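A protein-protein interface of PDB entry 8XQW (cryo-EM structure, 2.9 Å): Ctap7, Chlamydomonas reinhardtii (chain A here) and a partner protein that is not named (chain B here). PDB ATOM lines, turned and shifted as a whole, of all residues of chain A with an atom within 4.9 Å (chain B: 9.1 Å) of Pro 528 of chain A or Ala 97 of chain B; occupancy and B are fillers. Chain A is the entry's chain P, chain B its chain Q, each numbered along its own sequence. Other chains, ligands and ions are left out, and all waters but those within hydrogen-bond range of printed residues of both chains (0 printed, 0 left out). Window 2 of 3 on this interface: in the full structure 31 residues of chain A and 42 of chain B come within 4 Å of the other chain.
Pro 528 of chain A touches just one residue of chain B: Ala 97.
Ala 97 of chain B touches just these residues of chain A: Pro 522 (3.4 Å), Pro 528 (3.6 Å) and Phe 530 (3.9 Å).
No residue of chain B comes within 4 Å of Ser 529 of chain A.
Of the printed residues of chain A, Ser 336 of chain B touches Asn 523.
Of the printed residues of chain A, Leu 341 of chain B touches Pro 522.
Printed residues of chain A within 4 Å of Met 96 of chain B: Pro 522 (3.7 Å) and Asn 523 (3.2 Å).
Printed residues of chain B within 4 Å of Pro 522 of chain A: Met 96 (3.7 Å), Ala 97 (3.4 Å) and Leu 341 (3.7 Å).
Ala 103 of chain B touches none of the printed residues of chain A.
The nearest residue of chain A that does not touch Ala 97 of chain B is Asn 523 of chain A (4.5 Å).
The nearest printed residue of chain A that does not touch Met 96 of chain B is Pro 528 of chain A (6.2 Å).
Of the 17 printed residues of chain B, 7 touch a printed residue of chain A.
Of the 9 printed residues of chain A, 4 touch a printed residue of chain B.
Printed residues of chain A that touch a printed residue of chain B: Pro 522, Asn 523, Pro 528 and Phe 530.
Among the printed residues, no Asp or Glu carboxylate lies within 4 Å of a Lys or Arg side-chain nitrogen of the other chain.
C of Met 96 of chain B touches O of Pro 522 of chain A, 3.7 Å away.
Leu 341 of chain B touches Pro 522 of chain A (CD2 to CG, 3.7 Å).
Thr 334 of chain B touches Asn 523 of chain A (O to OD1, 3.6 Å).
CB of Ala 337 of chain B touches ND2 of Asn 523 of chain A, 3.8 Å away.
Pro 528 of chain A touches Ala 97 of chain B.
CE1 of Phe 530 of chain A touches CB of Ala 97 of chain B, 3.9 Å away.
Phe 530 of chain A touches Glu 100 of chain B (CB to OE2, 3.4 Å).
The backbone NH (N) of Met 96 of chain B sits at hydrogen-bond distance from the backbone carbonyl oxygen (O) of Thr 334 of chain B.
N of Met 96 of chain B sits at hydrogen-bond distance from O of Ser 336 of chain B, at 2.6 Å.
The backbone carbonyl oxygen (O) of Glu 100 of chain B lies close to the guanidinium group (NH1) of Arg 104 of chain B, 3.4 Å away.
The backbone NH (N) of Leu 341 of chain B sits at hydrogen-bond distance from the side-chain hydroxyl (OG) of Ser 336 of chain B, 3.5 Å away.
O of Leu 341 of chain B is in hydrogen-bond range of OG of Ser 345 of chain B.
The backbone carbonyl oxygen of Pro 522 of chain A sits at hydrogen-bond distance from the backbone NH of Ala 97 of chain B (3.4 Å).
N of Met 96 of chain B is in hydrogen-bond range of OD1 of Asn 523 of chain A.
The side-chain amide nitrogen (ND2) of Asn 523 of chain A sits at hydrogen-bond distance from the backbone carbonyl oxygen (O) of Ser 336 of chain B, 3.0 Å away.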
ATOM      1  N   ASP A 521     -23.836 -12.252 -24.232  1.00  0.00           N
ATOM      2  CA  ASP A 521     -25.150 -12.072 -24.826  1.00  0.00           C
ATOM      3  C   ASP A 521     -25.680 -10.700 -24.458  1.00  0.00           C
ATOM      4  O   ASP A 521     -25.786 -10.393 -23.262  1.00  0.00           O
ATOM      5  CB  ASP A 521     -26.105 -13.154 -24.341  1.00  0.00           C
ATOM      6  CG  ASP A 521     -27.280 -13.358 -25.274  1.00  0.00           C
ATOM      7  OD1 ASP A 521     -27.333 -12.691 -26.325  1.00  0.00           O
ATOM      8  OD2 ASP A 521     -28.151 -14.195 -24.964  1.00  0.00           O
ATOM      9  N   PRO A 522     -26.022  -9.849 -25.427  1.00  0.00           N
ATOM     10  CA  PRO A 522     -26.436  -8.478 -25.098  1.00  0.00           C
ATOM     11  C   PRO A 522     -27.739  -8.384 -24.328  1.00  0.00           C
ATOM     12  O   PRO A 522     -28.165  -7.265 -24.015  1.00  0.00           O
ATOM     13  CB  PRO A 522     -26.562  -7.812 -26.473  1.00  0.00           C
ATOM     14  CG  PRO A 522     -26.671  -8.929 -27.438  1.00  0.00           C
ATOM     15  CD  PRO A 522     -25.871 -10.043 -26.876  1.00  0.00           C
ATOM     16  N   ASN A 523     -28.389  -9.499 -24.009  1.00  0.00           N
ATOM     17  CA  ASN A 523     -29.642  -9.471 -23.273  1.00  0.00           C
ATOM     18  C   ASN A 523     -29.607 -10.346 -22.032  1.00  0.00           C
ATOM     19  O   ASN A 523     -30.636 -10.912 -21.652  1.00  0.00           O
ATOM     20  CB  ASN A 523     -30.798  -9.882 -24.185  1.00  0.00           C
ATOM     21  CG  ASN A 523     -31.232  -8.763 -25.110  1.00  0.00           C
ATOM     22  OD1 ASN A 523     -31.407  -7.624 -24.682  1.00  0.00           O
ATOM     23  ND2 ASN A 523     -31.403  -9.078 -26.386  1.00  0.00           N
ATOM     24  N   HIS A 524     -28.452 -10.479 -21.402  1.00  0.00           N
ATOM     25  CA  HIS A 524     -28.393 -11.170 -20.129  1.00  0.00           C
ATOM     26  C   HIS A 524     -29.103 -10.336 -19.067  1.00  0.00           C
ATOM     27  O   HIS A 524     -29.001  -9.107 -19.074  1.00  0.00           O
ATOM     28  CB  HIS A 524     -26.947 -11.415 -19.724  1.00  0.00           C
ATOM     29  CG  HIS A 524     -26.784 -12.398 -18.610  1.00  0.00           C
ATOM     30  ND1 HIS A 524     -26.826 -12.031 -17.284  1.00  0.00           N
ATOM     31  CD2 HIS A 524     -26.556 -13.731 -18.625  1.00  0.00           C
ATOM     32  CE1 HIS A 524     -26.638 -13.097 -16.529  1.00  0.00           C
ATOM     33  NE2 HIS A 524     -26.474 -14.143 -17.318  1.00  0.00           N
ATOM     34  N   LEU A 526     -28.593 -10.098 -15.724  1.00  0.00           N
ATOM     35  CA  LEU A 526     -27.702  -9.506 -14.733  1.00  0.00           C
ATOM     36  C   LEU A 526     -26.639  -8.620 -15.368  1.00  0.00           C
ATOM     37  O   LEU A 526     -26.621  -7.408 -15.146  1.00  0.00           O
ATOM     38  CB  LEU A 526     -27.020 -10.612 -13.921  1.00  0.00           C
ATOM     39  CG  LEU A 526     -27.703 -11.130 -12.667  1.00  0.00           C
ATOM     40  CD1 LEU A 526     -26.947 -12.329 -12.142  1.00  0.00           C
ATOM     41  CD2 LEU A 526     -27.767 -10.037 -11.630  1.00  0.00           C
ATOM     42  N   TYR A 527     -25.762  -9.206 -16.181  1.00  0.00           N
ATOM     43  CA  TYR A 527     -24.593  -8.527 -16.726  1.00  0.00           C
ATOM     44  C   TYR A 527     -24.656  -8.584 -18.245  1.00  0.00           C
ATOM     45  O   TYR A 527     -24.084  -9.493 -18.864  1.00  0.00           O
ATOM     46  CB  TYR A 527     -23.296  -9.155 -16.230  1.00  0.00           C
ATOM     47  CG  TYR A 527     -23.255  -9.455 -14.757  1.00  0.00           C
ATOM     48  CD1 TYR A 527     -23.298  -8.441 -13.821  1.00  0.00           C
ATOM     49  CD2 TYR A 527     -23.145 -10.755 -14.303  1.00  0.00           C
ATOM     50  CE1 TYR A 527     -23.250  -8.717 -12.475  1.00  0.00           C
ATOM     51  CE2 TYR A 527     -23.095 -11.040 -12.962  1.00  0.00           C
ATOM     52  CZ  TYR A 527     -23.149 -10.020 -12.052  1.00  0.00           C
ATOM     53  OH  TYR A 527     -23.099 -10.309 -10.713  1.00  0.00           O
ATOM     54  N   PRO A 528     -25.320  -7.630 -18.880  1.00  0.00           N
ATOM     55  CA  PRO A 528     -25.320  -7.584 -20.340  1.00  0.00           C
ATOM     56  C   PRO A 528     -23.921  -7.344 -20.871  1.00  0.00           C
ATOM     57  O   PRO A 528     -22.970  -7.120 -20.120  1.00  0.00           O
ATOM     58  CB  PRO A 528     -26.235  -6.397 -20.663  1.00  0.00           C
ATOM     59  CG  PRO A 528     -26.895  -6.030 -19.385  1.00  0.00           C
ATOM     60  CD  PRO A 528     -25.998  -6.469 -18.290  1.00  0.00           C
ATOM     61  N   SER A 529     -23.802  -7.398 -22.190  1.00  0.00           N
ATOM     62  CA  SER A 529     -22.564  -7.038 -22.864  1.00  0.00           C
ATOM     63  C   SER A 529     -22.850  -5.961 -23.895  1.00  0.00           C
ATOM     64  O   SER A 529     -23.580  -6.193 -24.861  1.00  0.00           O
ATOM     65  CB  SER A 529     -21.927  -8.250 -23.536  1.00  0.00           C
ATOM     66  OG  SER A 529     -22.613  -8.581 -24.728  1.00  0.00           O
ATOM     67  N   PHE A 530     -22.267  -4.787 -23.694  1.00  0.00           N
ATOM     68  CA  PHE A 530     -22.521  -3.648 -24.558  1.00  0.00           C
ATOM     69  C   PHE A 530     -21.873  -3.850 -25.918  1.00  0.00           C
ATOM     70  O   PHE A 530     -21.008  -4.702 -26.112  1.00  0.00           O
ATOM     71  CB  PHE A 530     -21.992  -2.361 -23.929  1.00  0.00           C
ATOM     72  CG  PHE A 530     -22.469  -2.131 -22.537  1.00  0.00           C
ATOM     73  CD1 PHE A 530     -23.814  -2.164 -22.240  1.00  0.00           C
ATOM     74  CD2 PHE A 530     -21.569  -1.886 -21.522  1.00  0.00           C
ATOM     75  CE1 PHE A 530     -24.255  -1.953 -20.955  1.00  0.00           C
ATOM     76  CE2 PHE A 530     -22.004  -1.675 -20.238  1.00  0.00           C
ATOM     77  CZ  PHE A 530     -23.348  -1.708 -19.953  1.00  0.00           C
ATOM     78  N   MET B  96     -30.681  -5.494 -26.990  1.00  0.00           N
ATOM     79  CA  MET B  96     -29.871  -4.374 -26.526  1.00  0.00           C
ATOM     80  C   MET B  96     -30.017  -4.179 -25.021  1.00  0.00           C
ATOM     81  O   MET B  96     -31.118  -4.248 -24.482  1.00  0.00           O
ATOM     82  CB  MET B  96     -30.258  -3.094 -27.268  1.00  0.00           C
ATOM     83  CG  MET B  96     -29.480  -1.877 -26.829  1.00  0.00           C
ATOM     84  SD  MET B  96     -28.704  -1.010 -28.201  1.00  0.00           S
ATOM     85  CE  MET B  96     -30.110  -0.176 -28.917  1.00  0.00           C
ATOM     86  N   ALA B  97     -28.892  -3.947 -24.350  1.00  0.00           N
ATOM     87  CA  ALA B  97     -28.905  -3.697 -22.918  1.00  0.00           C
ATOM     88  C   ALA B  97     -29.725  -2.456 -22.604  1.00  0.00           C
ATOM     89  O   ALA B  97     -29.823  -1.533 -23.414  1.00  0.00           O
ATOM     90  CB  ALA B  97     -27.479  -3.525 -22.398  1.00  0.00           C
ATOM     91  N   LYS B  98     -30.311  -2.437 -21.405  1.00  0.00           N
ATOM     92  CA  LYS B  98     -31.198  -1.339 -21.034  1.00  0.00           C
ATOM     93  C   LYS B  98     -30.468  -0.003 -21.059  1.00  0.00           C
ATOM     94  O   LYS B  98     -31.013   1.008 -21.521  1.00  0.00           O
ATOM     95  CB  LYS B  98     -31.797  -1.595 -19.652  1.00  0.00           C
ATOM     96  CG  LYS B  98     -32.868  -0.596 -19.260  1.00  0.00           C
ATOM     97  CD  LYS B  98     -33.719  -1.087 -18.102  1.00  0.00           C
ATOM     98  CE  LYS B  98     -33.000  -0.936 -16.774  1.00  0.00           C
ATOM     99  NZ  LYS B  98     -33.929  -1.101 -15.620  1.00  0.00           N
ATOM    100  N   ASP B  99     -29.226   0.015 -20.578  1.00  0.00           N
ATOM    101  CA  ASP B  99     -28.501   1.269 -20.442  1.00  0.00           C
ATOM    102  C   ASP B  99     -28.277   1.943 -21.786  1.00  0.00           C
ATOM    103  O   ASP B  99     -28.364   3.172 -21.884  1.00  0.00           O
ATOM    104  CB  ASP B  99     -27.173   1.006 -19.745  1.00  0.00           C
ATOM    105  CG  ASP B  99     -27.310   0.020 -18.606  1.00  0.00           C
ATOM    106  OD1 ASP B  99     -27.992  -1.008 -18.796  1.00  0.00           O
ATOM    107  OD2 ASP B  99     -26.748   0.269 -17.520  1.00  0.00           O
ATOM    108  N   GLU B 100     -28.009   1.163 -22.834  1.00  0.00           N
ATOM    109  CA  GLU B 100     -27.779   1.754 -24.146  1.00  0.00           C
ATOM    110  C   GLU B 100     -29.061   2.350 -24.704  1.00  0.00           C
ATOM    111  O   GLU B 100     -29.048   3.428 -25.311  1.00  0.00           O
ATOM    112  CB  GLU B 100     -27.205   0.706 -25.093  1.00  0.00           C
ATOM    113  CG  GLU B 100     -26.071  -0.103 -24.495  1.00  0.00           C
ATOM    114  CD  GLU B 100     -24.777   0.684 -24.372  1.00  0.00           C
ATOM    115  OE1 GLU B 100     -24.734   1.653 -23.587  1.00  0.00           O
ATOM    116  OE2 GLU B 100     -23.799   0.333 -25.066  1.00  0.00           O
ATOM    117  N   VAL B 101     -30.186   1.661 -24.502  1.00  0.00           N
ATOM    118  CA  VAL B 101     -31.469   2.218 -24.912  1.00  0.00           C
ATOM    119  C   VAL B 101     -31.718   3.536 -24.203  1.00  0.00           C
ATOM    120  O   VAL B 101     -32.131   4.524 -24.822  1.00  0.00           O
ATOM    121  CB  VAL B 101     -32.605   1.216 -24.643  1.00  0.00           C
ATOM    122  CG1 VAL B 101     -33.832   1.606 -25.433  1.00  0.00           C
ATOM    123  CG2 VAL B 101     -32.172  -0.183 -25.001  1.00  0.00           C
ATOM    124  N   LYS B 102     -31.462   3.575 -22.896  1.00  0.00           N
ATOM    125  CA  LYS B 102     -31.655   4.812 -22.153  1.00  0.00           C
ATOM    126  C   LYS B 102     -30.758   5.921 -22.686  1.00  0.00           C
ATOM    127  O   LYS B 102     -31.200   7.063 -22.843  1.00  0.00           O
ATOM    128  CB  LYS B 102     -31.402   4.574 -20.667  1.00  0.00           C
ATOM    129  CG  LYS B 102     -32.525   3.829 -19.980  1.00  0.00           C
ATOM    130  CD  LYS B 102     -32.048   3.160 -18.713  1.00  0.00           C
ATOM    131  CE  LYS B 102     -31.268   4.123 -17.842  1.00  0.00           C
ATOM    132  NZ  LYS B 102     -30.582   3.406 -16.737  1.00  0.00           N
ATOM    133  N   ALA B 103     -29.501   5.601 -22.986  1.00  0.00           N
ATOM    134  CA  ALA B 103     -28.599   6.605 -23.527  1.00  0.00           C
ATOM    135  C   ALA B 103     -29.005   7.064 -24.918  1.00  0.00           C
ATOM    136  O   ALA B 103     -28.624   8.163 -25.328  1.00  0.00           O
ATOM    137  CB  ALA B 103     -27.172   6.067 -23.561  1.00  0.00           C
ATOM    138  N   ARG B 104     -29.762   6.252 -25.651  1.00  0.00           N
ATOM    139  CA  ARG B 104     -30.136   6.633 -27.007  1.00  0.00           C
ATOM    140  C   ARG B 104     -31.425   7.443 -27.055  1.00  0.00           C
ATOM    141  O   ARG B 104     -31.682   8.121 -28.054  1.00  0.00           O
ATOM    142  CB  ARG B 104     -30.267   5.390 -27.883  1.00  0.00           C
ATOM    143  CG  ARG B 104     -28.969   4.979 -28.537  1.00  0.00           C
ATOM    144  CD  ARG B 104     -28.955   3.508 -28.878  1.00  0.00           C
ATOM    145  NE  ARG B 104     -27.706   3.126 -29.527  1.00  0.00           N
ATOM    146  CZ  ARG B 104     -26.582   2.852 -28.875  1.00  0.00           C
ATOM    147  NH1 ARG B 104     -26.549   2.918 -27.552  1.00  0.00           N
ATOM    148  NH2 ARG B 104     -25.493   2.512 -29.543  1.00  0.00           N
ATOM    149  N   TYR B 170     -38.937   6.153 -19.684  1.00  0.00           N
ATOM    150  CA  TYR B 170     -38.671   4.773 -20.068  1.00  0.00           C
ATOM    151  C   TYR B 170     -38.372   3.934 -18.838  1.00  0.00           C
ATOM    152  O   TYR B 170     -38.871   2.814 -18.697  1.00  0.00           O
ATOM    153  CB  TYR B 170     -37.510   4.697 -21.058  1.00  0.00           C
ATOM    154  CG  TYR B 170     -37.010   3.284 -21.272  1.00  0.00           C
ATOM    155  CD1 TYR B 170     -37.636   2.438 -22.173  1.00  0.00           C
ATOM    156  CD2 TYR B 170     -35.923   2.790 -20.562  1.00  0.00           C
ATOM    157  CE1 TYR B 170     -37.193   1.145 -22.366  1.00  0.00           C
ATOM    158  CE2 TYR B 170     -35.476   1.500 -20.749  1.00  0.00           C
ATOM    159  CZ  TYR B 170     -36.114   0.682 -21.650  1.00  0.00           C
ATOM    160  OH  TYR B 170     -35.669  -0.603 -21.839  1.00  0.00           O
ATOM    161  N   MET B 333     -36.295  -2.046 -30.152  1.00  0.00           N
ATOM    162  CA  MET B 333     -34.967  -1.631 -29.721  1.00  0.00           C
ATOM    163  C   MET B 333     -34.528  -2.397 -28.484  1.00  0.00           C
ATOM    164  O   MET B 333     -33.384  -2.855 -28.405  1.00  0.00           O
ATOM    165  CB  MET B 333     -34.960  -0.129 -29.446  1.00  0.00           C
ATOM    166  CG  MET B 333     -33.655   0.566 -29.739  1.00  0.00           C
ATOM    167  SD  MET B 333     -33.819   2.351 -29.579  1.00  0.00           S
ATOM    168  CE  MET B 333     -32.340   2.906 -30.417  1.00  0.00           C
ATOM    169  N   THR B 334     -35.426  -2.554 -27.514  1.00  0.00           N
ATOM    170  CA  THR B 334     -35.059  -3.225 -26.272  1.00  0.00           C
ATOM    171  C   THR B 334     -34.746  -4.698 -26.505  1.00  0.00           C
ATOM    172  O   THR B 334     -33.660  -5.174 -26.163  1.00  0.00           O
ATOM    173  CB  THR B 334     -36.168  -3.063 -25.235  1.00  0.00           C
ATOM    174  OG1 THR B 334     -37.344  -3.747 -25.683  1.00  0.00           O
ATOM    175  CG2 THR B 334     -36.474  -1.593 -25.000  1.00  0.00           C
ATOM    176  N   ALA B 335     -35.685  -5.441 -27.079  1.00  0.00           N
ATOM    177  CA  ALA B 335     -35.489  -6.874 -27.290  1.00  0.00           C
ATOM    178  C   ALA B 335     -34.819  -7.166 -28.628  1.00  0.00           C
ATOM    179  O   ALA B 335     -35.305  -7.964 -29.425  1.00  0.00           O
ATOM    180  CB  ALA B 335     -36.820  -7.603 -27.179  1.00  0.00           C
ATOM    181  N   SER B 336     -33.682  -6.528 -28.874  1.00  0.00           N
ATOM    182  CA  SER B 336     -32.936  -6.696 -30.111  1.00  0.00           C
ATOM    183  C   SER B 336     -31.640  -7.453 -29.850  1.00  0.00           C
ATOM    184  O   SER B 336     -31.042  -7.340 -28.777  1.00  0.00           O
ATOM    185  CB  SER B 336     -32.620  -5.341 -30.748  1.00  0.00           C
ATOM    186  OG  SER B 336     -32.564  -5.445 -32.156  1.00  0.00           O
ATOM    187  N   ALA B 337     -31.209  -8.222 -30.850  1.00  0.00           N
ATOM    188  CA  ALA B 337     -29.970  -8.988 -30.760  1.00  0.00           C
ATOM    189  C   ALA B 337     -29.610  -9.499 -32.145  1.00  0.00           C
ATOM    190  O   ALA B 337     -30.487  -9.952 -32.883  1.00  0.00           O
ATOM    191  CB  ALA B 337     -30.104 -10.159 -29.779  1.00  0.00           C
ATOM    192  N   LEU B 341     -29.715  -5.847 -34.137  1.00  0.00           N
ATOM    193  CA  LEU B 341     -29.023  -5.108 -33.087  1.00  0.00           C
ATOM    194  C   LEU B 341     -28.008  -4.144 -33.679  1.00  0.00           C
ATOM    195  O   LEU B 341     -27.943  -2.975 -33.281  1.00  0.00           O
ATOM    196  CB  LEU B 341     -28.338  -6.080 -32.131  1.00  0.00           C
ATOM    197  CG  LEU B 341     -27.390  -5.454 -31.110  1.00  0.00           C
ATOM    198  CD1 LEU B 341     -28.103  -4.377 -30.320  1.00  0.00           C
ATOM    199  CD2 LEU B 341     -26.838  -6.518 -30.183  1.00  0.00           C
ATOM    200  N   SER B 345     -28.077  -0.070 -33.434  1.00  0.00           N
ATOM    201  CA  SER B 345     -26.998   0.559 -32.686  1.00  0.00           C
ATOM    202  C   SER B 345     -26.533   1.875 -33.294  1.00  0.00           C
ATOM    203  O   SER B 345     -25.604   2.488 -32.764  1.00  0.00           O
ATOM    204  CB  SER B 345     -25.822  -0.406 -32.577  1.00  0.00           C
ATOM    205  OG  SER B 345     -26.065  -1.368 -31.569  1.00  0.00           O
